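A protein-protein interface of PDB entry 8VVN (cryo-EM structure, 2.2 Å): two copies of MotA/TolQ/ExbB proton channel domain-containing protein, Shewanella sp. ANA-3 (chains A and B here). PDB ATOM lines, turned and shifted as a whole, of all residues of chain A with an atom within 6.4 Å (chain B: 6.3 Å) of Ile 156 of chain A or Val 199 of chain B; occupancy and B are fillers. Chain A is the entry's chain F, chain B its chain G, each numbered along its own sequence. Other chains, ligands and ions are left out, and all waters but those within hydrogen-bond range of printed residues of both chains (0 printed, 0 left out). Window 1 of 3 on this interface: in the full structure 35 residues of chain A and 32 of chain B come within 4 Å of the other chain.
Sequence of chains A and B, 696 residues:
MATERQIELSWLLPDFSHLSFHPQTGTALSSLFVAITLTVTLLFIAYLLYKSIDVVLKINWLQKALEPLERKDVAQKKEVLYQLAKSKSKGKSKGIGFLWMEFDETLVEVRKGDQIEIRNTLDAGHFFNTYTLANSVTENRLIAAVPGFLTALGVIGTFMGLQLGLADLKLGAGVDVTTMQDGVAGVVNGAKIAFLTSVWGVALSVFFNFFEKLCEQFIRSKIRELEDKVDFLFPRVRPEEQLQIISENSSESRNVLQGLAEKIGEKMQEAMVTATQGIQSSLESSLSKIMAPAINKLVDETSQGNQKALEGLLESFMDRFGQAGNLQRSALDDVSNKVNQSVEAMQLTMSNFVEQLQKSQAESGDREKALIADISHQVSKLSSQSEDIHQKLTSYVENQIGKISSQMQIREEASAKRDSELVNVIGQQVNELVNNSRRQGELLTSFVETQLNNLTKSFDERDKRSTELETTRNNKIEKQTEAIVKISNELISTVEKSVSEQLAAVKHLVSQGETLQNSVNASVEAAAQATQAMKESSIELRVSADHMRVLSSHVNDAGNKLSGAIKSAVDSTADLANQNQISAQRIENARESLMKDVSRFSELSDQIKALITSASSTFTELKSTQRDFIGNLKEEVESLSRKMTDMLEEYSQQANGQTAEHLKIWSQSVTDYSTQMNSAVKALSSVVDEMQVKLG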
ATOM      1  N   PHE A  33      -5.530  -6.812  24.486  1.00  0.00           N
ATOM      2  CA  PHE A  33      -6.118  -6.434  25.763  1.00  0.00           C
ATOM      3  C   PHE A  33      -5.648  -7.360  26.877  1.00  0.00           C
ATOM      4  O   PHE A  33      -5.362  -6.908  27.990  1.00  0.00           O
ATOM      5  CB  PHE A  33      -7.638  -6.454  25.655  1.00  0.00           C
ATOM      6  CG  PHE A  33      -8.315  -5.529  26.600  1.00  0.00           C
ATOM      7  CD1 PHE A  33      -8.560  -5.910  27.900  1.00  0.00           C
ATOM      8  CD2 PHE A  33      -8.720  -4.274  26.182  1.00  0.00           C
ATOM      9  CE1 PHE A  33      -9.174  -5.054  28.769  1.00  0.00           C
ATOM     10  CE2 PHE A  33      -9.349  -3.413  27.049  1.00  0.00           C
ATOM     11  CZ  PHE A  33      -9.574  -3.801  28.344  1.00  0.00           C
ATOM     12  N   PHE A 149      -7.869  -2.714  39.627  1.00  0.00           N
ATOM     13  CA  PHE A 149      -7.436  -2.301  38.295  1.00  0.00           C
ATOM     14  C   PHE A 149      -7.643  -3.419  37.281  1.00  0.00           C
ATOM     15  O   PHE A 149      -8.186  -3.196  36.195  1.00  0.00           O
ATOM     16  CB  PHE A 149      -5.960  -1.891  38.306  1.00  0.00           C
ATOM     17  CG  PHE A 149      -5.647  -0.712  39.178  1.00  0.00           C
ATOM     18  CD1 PHE A 149      -6.597   0.258  39.441  1.00  0.00           C
ATOM     19  CD2 PHE A 149      -4.382  -0.571  39.728  1.00  0.00           C
ATOM     20  CE1 PHE A 149      -6.294   1.338  40.241  1.00  0.00           C
ATOM     21  CE2 PHE A 149      -4.075   0.508  40.527  1.00  0.00           C
ATOM     22  CZ  PHE A 149      -5.033   1.461  40.783  1.00  0.00           C
ATOM     23  N   THR A 151      -9.537  -6.193  37.436  1.00  0.00           N
ATOM     24  CA  THR A 151     -10.947  -6.495  37.229  1.00  0.00           C
ATOM     25  C   THR A 151     -11.607  -5.444  36.345  1.00  0.00           C
ATOM     26  O   THR A 151     -12.399  -5.773  35.457  1.00  0.00           O
ATOM     27  CB  THR A 151     -11.668  -6.589  38.575  1.00  0.00           C
ATOM     28  OG1 THR A 151     -11.193  -7.730  39.295  1.00  0.00           O
ATOM     29  CG2 THR A 151     -13.160  -6.720  38.377  1.00  0.00           C
ATOM     30  N   ALA A 152     -11.286  -4.172  36.572  1.00  0.00           N
ATOM     31  CA  ALA A 152     -11.880  -3.112  35.773  1.00  0.00           C
ATOM     32  C   ALA A 152     -11.340  -3.107  34.351  1.00  0.00           C
ATOM     33  O   ALA A 152     -12.054  -2.713  33.424  1.00  0.00           O
ATOM     34  CB  ALA A 152     -11.650  -1.768  36.447  1.00  0.00           C
ATOM     35  N   LEU A 153     -10.090  -3.532  34.157  1.00  0.00           N
ATOM     36  CA  LEU A 153      -9.598  -3.767  32.805  1.00  0.00           C
ATOM     37  C   LEU A 153     -10.481  -4.776  32.082  1.00  0.00           C
ATOM     38  O   LEU A 153     -10.968  -4.510  30.979  1.00  0.00           O
ATOM     39  CB  LEU A 153      -8.148  -4.245  32.842  1.00  0.00           C
ATOM     40  CG  LEU A 153      -7.069  -3.187  33.054  1.00  0.00           C
ATOM     41  CD1 LEU A 153      -5.692  -3.773  32.799  1.00  0.00           C
ATOM     42  CD2 LEU A 153      -7.316  -1.993  32.149  1.00  0.00           C
ATOM     43  N   GLY A 154     -10.736  -5.924  32.712  1.00  0.00           N
ATOM     44  CA  GLY A 154     -11.618  -6.907  32.108  1.00  0.00           C
ATOM     45  C   GLY A 154     -13.006  -6.361  31.838  1.00  0.00           C
ATOM     46  O   GLY A 154     -13.630  -6.701  30.834  1.00  0.00           O
ATOM     47  N   VAL A 155     -13.507  -5.506  32.730  1.00  0.00           N
ATOM     48  CA  VAL A 155     -14.801  -4.867  32.511  1.00  0.00           C
ATOM     49  C   VAL A 155     -14.737  -3.919  31.316  1.00  0.00           C
ATOM     50  O   VAL A 155     -15.672  -3.849  30.512  1.00  0.00           O
ATOM     51  CB  VAL A 155     -15.256  -4.147  33.794  1.00  0.00           C
ATOM     52  CG1 VAL A 155     -16.328  -3.113  33.487  1.00  0.00           C
ATOM     53  CG2 VAL A 155     -15.741  -5.153  34.825  1.00  0.00           C
ATOM     54  N   ILE A 156     -13.634  -3.179  31.180  1.00  0.00           N
ATOM     55  CA  ILE A 156     -13.461  -2.288  30.034  1.00  0.00           C
ATOM     56  C   ILE A 156     -13.477  -3.084  28.738  1.00  0.00           C
ATOM     57  O   ILE A 156     -14.087  -2.673  27.745  1.00  0.00           O
ATOM     58  CB  ILE A 156     -12.161  -1.476  30.182  1.00  0.00           C
ATOM     59  CG1 ILE A 156     -12.316  -0.403  31.258  1.00  0.00           C
ATOM     60  CG2 ILE A 156     -11.772  -0.837  28.861  1.00  0.00           C
ATOM     61  CD1 ILE A 156     -11.008   0.159  31.727  1.00  0.00           C
ATOM     62  N   GLY A 157     -12.811  -4.243  28.732  1.00  0.00           N
ATOM     63  CA  GLY A 157     -12.823  -5.092  27.557  1.00  0.00           C
ATOM     64  C   GLY A 157     -14.208  -5.579  27.185  1.00  0.00           C
ATOM     65  O   GLY A 157     -14.501  -5.773  26.005  1.00  0.00           O
ATOM     66  N   THR A 158     -15.072  -5.794  28.179  1.00  0.00           N
ATOM     67  CA  THR A 158     -16.447  -6.186  27.884  1.00  0.00           C
ATOM     68  C   THR A 158     -17.205  -5.084  27.160  1.00  0.00           C
ATOM     69  O   THR A 158     -17.785  -5.318  26.095  1.00  0.00           O
ATOM     70  CB  THR A 158     -17.182  -6.569  29.164  1.00  0.00           C
ATOM     71  OG1 THR A 158     -16.521  -7.674  29.788  1.00  0.00           O
ATOM     72  CG2 THR A 158     -18.626  -6.929  28.858  1.00  0.00           C
ATOM     73  N   PHE A 159     -17.219  -3.876  27.724  1.00  0.00           N
ATOM     74  CA  PHE A 159     -17.979  -2.801  27.098  1.00  0.00           C
ATOM     75  C   PHE A 159     -17.358  -2.387  25.776  1.00  0.00           C
ATOM     76  O   PHE A 159     -18.079  -2.021  24.844  1.00  0.00           O
ATOM     77  CB  PHE A 159     -18.100  -1.609  28.043  1.00  0.00           C
ATOM     78  CG  PHE A 159     -18.921  -1.896  29.262  1.00  0.00           C
ATOM     79  CD1 PHE A 159     -20.241  -2.287  29.140  1.00  0.00           C
ATOM     80  CD2 PHE A 159     -18.381  -1.766  30.528  1.00  0.00           C
ATOM     81  CE1 PHE A 159     -21.003  -2.557  30.255  1.00  0.00           C
ATOM     82  CE2 PHE A 159     -19.142  -2.030  31.647  1.00  0.00           C
ATOM     83  CZ  PHE A 159     -20.452  -2.427  31.510  1.00  0.00           C
ATOM     84  N   MET A 160     -16.033  -2.446  25.675  1.00  0.00           N
ATOM     85  CA  MET A 160     -15.375  -2.235  24.394  1.00  0.00           C
ATOM     86  C   MET A 160     -15.782  -3.307  23.389  1.00  0.00           C
ATOM     87  O   MET A 160     -16.157  -2.998  22.254  1.00  0.00           O
ATOM     88  CB  MET A 160     -13.861  -2.222  24.593  1.00  0.00           C
ATOM     89  CG  MET A 160     -13.073  -1.897  23.356  1.00  0.00           C
ATOM     90  SD  MET A 160     -11.302  -1.886  23.677  1.00  0.00           S
ATOM     91  CE  MET A 160     -11.165  -0.384  24.639  1.00  0.00           C
ATOM     92  N   GLY A 161     -15.721  -4.575  23.797  1.00  0.00           N
ATOM     93  CA  GLY A 161     -16.069  -5.652  22.885  1.00  0.00           C
ATOM     94  C   GLY A 161     -17.530  -5.627  22.477  1.00  0.00           C
ATOM     95  O   GLY A 161     -17.858  -5.764  21.297  1.00  0.00           O
ATOM     96  N   GLN A 163     -19.648  -3.062  22.537  1.00  0.00           N
ATOM     97  CA  GLN A 163     -19.934  -1.887  21.720  1.00  0.00           C
ATOM     98  C   GLN A 163     -19.475  -2.090  20.282  1.00  0.00           C
ATOM     99  O   GLN A 163     -20.189  -1.730  19.339  1.00  0.00           O
ATOM    100  CB  GLN A 163     -19.270  -0.651  22.322  1.00  0.00           C
ATOM    101  CG  GLN A 163     -19.214   0.546  21.400  1.00  0.00           C
ATOM    102  CD  GLN A 163     -20.553   1.231  21.266  1.00  0.00           C
ATOM    103  OE1 GLN A 163     -21.387   1.161  22.164  1.00  0.00           O
ATOM    104  NE2 GLN A 163     -20.769   1.893  20.139  1.00  0.00           N
ATOM    105  N   THR A 197     -11.678 -11.215  27.750  1.00  0.00           N
ATOM    106  CA  THR A 197     -10.990 -10.236  28.585  1.00  0.00           C
ATOM    107  C   THR A 197     -11.475 -10.285  30.028  1.00  0.00           C
ATOM    108  O   THR A 197     -10.714  -9.961  30.944  1.00  0.00           O
ATOM    109  CB  THR A 197     -11.137  -8.823  28.006  1.00  0.00           C
ATOM    110  OG1 THR A 197     -12.518  -8.451  27.938  1.00  0.00           O
ATOM    111  CG2 THR A 197     -10.517  -8.742  26.621  1.00  0.00           C
ATOM    112  N   LEU B  12     -15.689   3.584  19.273  1.00  0.00           N
ATOM    113  CA  LEU B  12     -15.561   3.912  20.685  1.00  0.00           C
ATOM    114  C   LEU B  12     -15.386   5.402  20.933  1.00  0.00           C
ATOM    115  O   LEU B  12     -15.534   5.844  22.076  1.00  0.00           O
ATOM    116  CB  LEU B  12     -14.377   3.155  21.282  1.00  0.00           C
ATOM    117  CG  LEU B  12     -14.365   1.652  21.026  1.00  0.00           C
ATOM    118  CD1 LEU B  12     -13.055   1.062  21.494  1.00  0.00           C
ATOM    119  CD2 LEU B  12     -15.536   0.978  21.721  1.00  0.00           C
ATOM    120  N   ALA B 194     -25.562   2.577  26.261  1.00  0.00           N
ATOM    121  CA  ALA B 194     -25.200   2.066  27.576  1.00  0.00           C
ATOM    122  C   ALA B 194     -23.740   1.630  27.626  1.00  0.00           C
ATOM    123  O   ALA B 194     -23.025   1.943  28.582  1.00  0.00           O
ATOM    124  CB  ALA B 194     -26.122   0.911  27.956  1.00  0.00           C
ATOM    125  N   PHE B 195     -23.278   0.914  26.601  1.00  0.00           N
ATOM    126  CA  PHE B 195     -21.913   0.403  26.620  1.00  0.00           C
ATOM    127  C   PHE B 195     -20.885   1.479  26.302  1.00  0.00           C
ATOM    128  O   PHE B 195     -19.761   1.416  26.808  1.00  0.00           O
ATOM    129  CB  PHE B 195     -21.772  -0.775  25.655  1.00  0.00           C
ATOM    130  CG  PHE B 195     -22.745  -1.886  25.915  1.00  0.00           C
ATOM    131  CD1 PHE B 195     -23.162  -2.715  24.890  1.00  0.00           C
ATOM    132  CD2 PHE B 195     -23.243  -2.107  27.190  1.00  0.00           C
ATOM    133  CE1 PHE B 195     -24.055  -3.734  25.128  1.00  0.00           C
ATOM    134  CE2 PHE B 195     -24.138  -3.125  27.432  1.00  0.00           C
ATOM    135  CZ  PHE B 195     -24.544  -3.942  26.400  1.00  0.00           C
ATOM    136  N   LEU B 196     -21.241   2.460  25.470  1.00  0.00           N
ATOM    137  CA  LEU B 196     -20.316   3.550  25.186  1.00  0.00           C
ATOM    138  C   LEU B 196     -20.068   4.399  26.426  1.00  0.00           C
ATOM    139  O   LEU B 196     -18.924   4.767  26.713  1.00  0.00           O
ATOM    140  CB  LEU B 196     -20.849   4.414  24.043  1.00  0.00           C
ATOM    141  CG  LEU B 196     -19.921   5.501  23.493  1.00  0.00           C
ATOM    142  CD1 LEU B 196     -18.475   5.022  23.442  1.00  0.00           C
ATOM    143  CD2 LEU B 196     -20.377   5.965  22.125  1.00  0.00           C
ATOM    144  N   THR B 197     -21.124   4.713  27.178  1.00  0.00           N
ATOM    145  CA  THR B 197     -20.941   5.479  28.405  1.00  0.00           C
ATOM    146  C   THR B 197     -20.245   4.650  29.476  1.00  0.00           C
ATOM    147  O   THR B 197     -19.465   5.191  30.267  1.00  0.00           O
ATOM    148  CB  THR B 197     -22.285   5.998  28.921  1.00  0.00           C
ATOM    149  OG1 THR B 197     -23.149   4.899  29.230  1.00  0.00           O
ATOM    150  CG2 THR B 197     -22.953   6.848  27.865  1.00  0.00           C
ATOM    151  N   SER B 198     -20.512   3.343  29.512  1.00  0.00           N
ATOM    152  CA  SER B 198     -19.879   2.477  30.502  1.00  0.00           C
ATOM    153  C   SER B 198     -18.380   2.356  30.266  1.00  0.00           C
ATOM    154  O   SER B 198     -17.595   2.424  31.217  1.00  0.00           O
ATOM    155  CB  SER B 198     -20.522   1.093  30.484  1.00  0.00           C
ATOM    156  OG  SER B 198     -21.878   1.152  30.871  1.00  0.00           O
ATOM    157  N   VAL B 199     -17.961   2.166  29.013  1.00  0.00           N
ATOM    158  CA  VAL B 199     -16.544   1.938  28.754  1.00  0.00           C
ATOM    159  C   VAL B 199     -15.738   3.181  29.105  1.00  0.00           C
ATOM    160  O   VAL B 199     -14.627   3.084  29.634  1.00  0.00           O
ATOM    161  CB  VAL B 199     -16.315   1.484  27.296  1.00  0.00           C
ATOM    162  CG1 VAL B 199     -16.682   2.568  26.298  1.00  0.00           C
ATOM    163  CG2 VAL B 199     -14.883   1.014  27.098  1.00  0.00           C
ATOM    164  N   TRP B 200     -16.293   4.365  28.848  1.00  0.00           N
ATOM    165  CA  TRP B 200     -15.614   5.595  29.227  1.00  0.00           C
ATOM    166  C   TRP B 200     -15.700   5.847  30.726  1.00  0.00           C
ATOM    167  O   TRP B 200     -14.722   6.284  31.337  1.00  0.00           O
ATOM    168  CB  TRP B 200     -16.194   6.773  28.452  1.00  0.00           C
ATOM    169  CG  TRP B 200     -15.670   6.834  27.072  1.00  0.00           C
ATOM    170  CD1 TRP B 200     -16.240   6.308  25.956  1.00  0.00           C
ATOM    171  CD2 TRP B 200     -14.445   7.433  26.655  1.00  0.00           C
ATOM    172  NE1 TRP B 200     -15.454   6.552  24.864  1.00  0.00           N
ATOM    173  CE2 TRP B 200     -14.343   7.244  25.266  1.00  0.00           C
ATOM    174  CE3 TRP B 200     -13.426   8.122  27.320  1.00  0.00           C
ATOM    175  CZ2 TRP B 200     -13.263   7.717  24.527  1.00  0.00           C
ATOM    176  CZ3 TRP B 200     -12.357   8.590  26.586  1.00  0.00           C
ATOM    177  CH2 TRP B 200     -12.282   8.385  25.203  1.00  0.00           C
ATOM    178  N   GLY B 201     -16.854   5.564  31.330  1.00  0.00           N
ATOM    179  CA  GLY B 201     -16.987   5.746  32.764  1.00  0.00           C
ATOM    180  C   GLY B 201     -16.023   4.878  33.548  1.00  0.00           C
ATOM    181  O   GLY B 201     -15.356   5.348  34.471  1.00  0.00           O
ATOM    182  N   VAL B 202     -15.929   3.599  33.186  1.00  0.00           N
ATOM    183  CA  VAL B 202     -15.014   2.700  33.882  1.00  0.00           C
ATOM    184  C   VAL B 202     -13.567   3.073  33.581  1.00  0.00           C
ATOM    185  O   VAL B 202     -12.752   3.216  34.496  1.00  0.00           O
ATOM    186  CB  VAL B 202     -15.311   1.234  33.520  1.00  0.00           C
ATOM    187  CG1 VAL B 202     -14.318   0.309  34.208  1.00  0.00           C
ATOM    188  CG2 VAL B 202     -16.730   0.871  33.914  1.00  0.00           C
ATOM    189  N   ALA B 203     -13.237   3.283  32.304  1.00  0.00           N
ATOM    190  CA  ALA B 203     -11.851   3.567  31.938  1.00  0.00           C
ATOM    191  C   ALA B 203     -11.349   4.838  32.606  1.00  0.00           C
ATOM    192  O   ALA B 203     -10.214   4.886  33.090  1.00  0.00           O
ATOM    193  CB  ALA B 203     -11.705   3.676  30.422  1.00  0.00           C
ATOM    194  N   LEU B 204     -12.179   5.878  32.639  1.00  0.00           N
ATOM    195  CA  LEU B 204     -11.769   7.124  33.273  1.00  0.00           C
ATOM    196  C   LEU B 204     -11.680   6.957  34.783  1.00  0.00           C
ATOM    197  O   LEU B 204     -10.789   7.524  35.425  1.00  0.00           O
ATOM    198  CB  LEU B 204     -12.748   8.233  32.902  1.00  0.00           C
ATOM    199  CG  LEU B 204     -12.458   8.963  31.589  1.00  0.00           C
ATOM    200  CD1 LEU B 204     -13.603   9.894  31.252  1.00  0.00           C
ATOM    201  CD2 LEU B 204     -11.133   9.700  31.595  1.00  0.00           C
ATOM    202  N   VAL B 206     -10.904   4.142  36.405  1.00  0.00           N
ATOM    203  CA  VAL B 206      -9.671   3.407  36.682  1.00  0.00           C
ATOM    204  C   VAL B 206      -8.463   4.303  36.491  1.00  0.00           C
ATOM    205  O   VAL B 206      -7.513   4.264  37.281  1.00  0.00           O
ATOM    206  CB  VAL B 206      -9.571   2.154  35.794  1.00  0.00           C
ATOM    207  CG1 VAL B 206      -8.422   1.276  36.252  1.00  0.00           C
ATOM    208  CG2 VAL B 206     -10.842   1.402  35.849  1.00  0.00           C
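Of the printed residues of chain B, Phe 149 of chain A touches Val 206. Ile 156 of chain A touches just these residues of chain B: Val 199, Val 202 and Ala 203. Of the printed residues of chain B, Met 160 of chain A touches Leu 12 and Val 199. Of the printed residues of chain B, Gln 163 of chain A touches Leu 12 and Leu 196. Printed residues of chain A within 4 Å of Phe 195 of chain B: Phe 159. Val 199 of chain B touches just these residues of chain A: Ile 156 (3.8 Å), Phe 159 (3.6 Å) and Met 160 (3.9 Å). Of the printed residues of chain A, Val 202 of chain B touches Ala 152 and Ile 156.
The backbone carbonyl oxygen of Ala 194 of chain B is in hydrogen-bond range of the side-chain hydroxyl of Ser 198 of chain B, 2.7 Å away. NE1 of Trp 200 of chain B is in hydrogen-bond range of O of Leu 12 of chain B (2.9 Å).
Position printed for both chains: 197.
Along chain A the printed residues that touch a printed residue of chain B span positions 149 to 163. Hydrophobic or aromatic side chains of chain B within 4 Å of the printed part of chain A: Leu 12, Phe 195, Leu 196, Val 199, Val 202, Ala 203 and Val 206.
Among the printed residues, pairs that only touch across the chains: Phe 149 of chain A with Val 206 of chain B, Ala 152 of chain A with Val 202 of chain B, Ala 152 of chain A with Val 206 of chain B, Ile 156 of chain A with Val 199 of chain B, Ile 156 of chain A with Val 202 of chain B, Ile 156 of chain A with Ala 203 of chain B, Phe 159 of chain A with Phe 195 of chain B, Phe 159 of chain A with Ser 198 of chain B, Phe 159 of chain A with Val 199 of chain B, Met 160 of chain A with Leu 12 of chain B, Met 160 of chain A with Val 199 of chain B, Gln 163 of chain A with Leu 12 of chain B and Gln 163 of chain A with Leu 196 of chain B.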
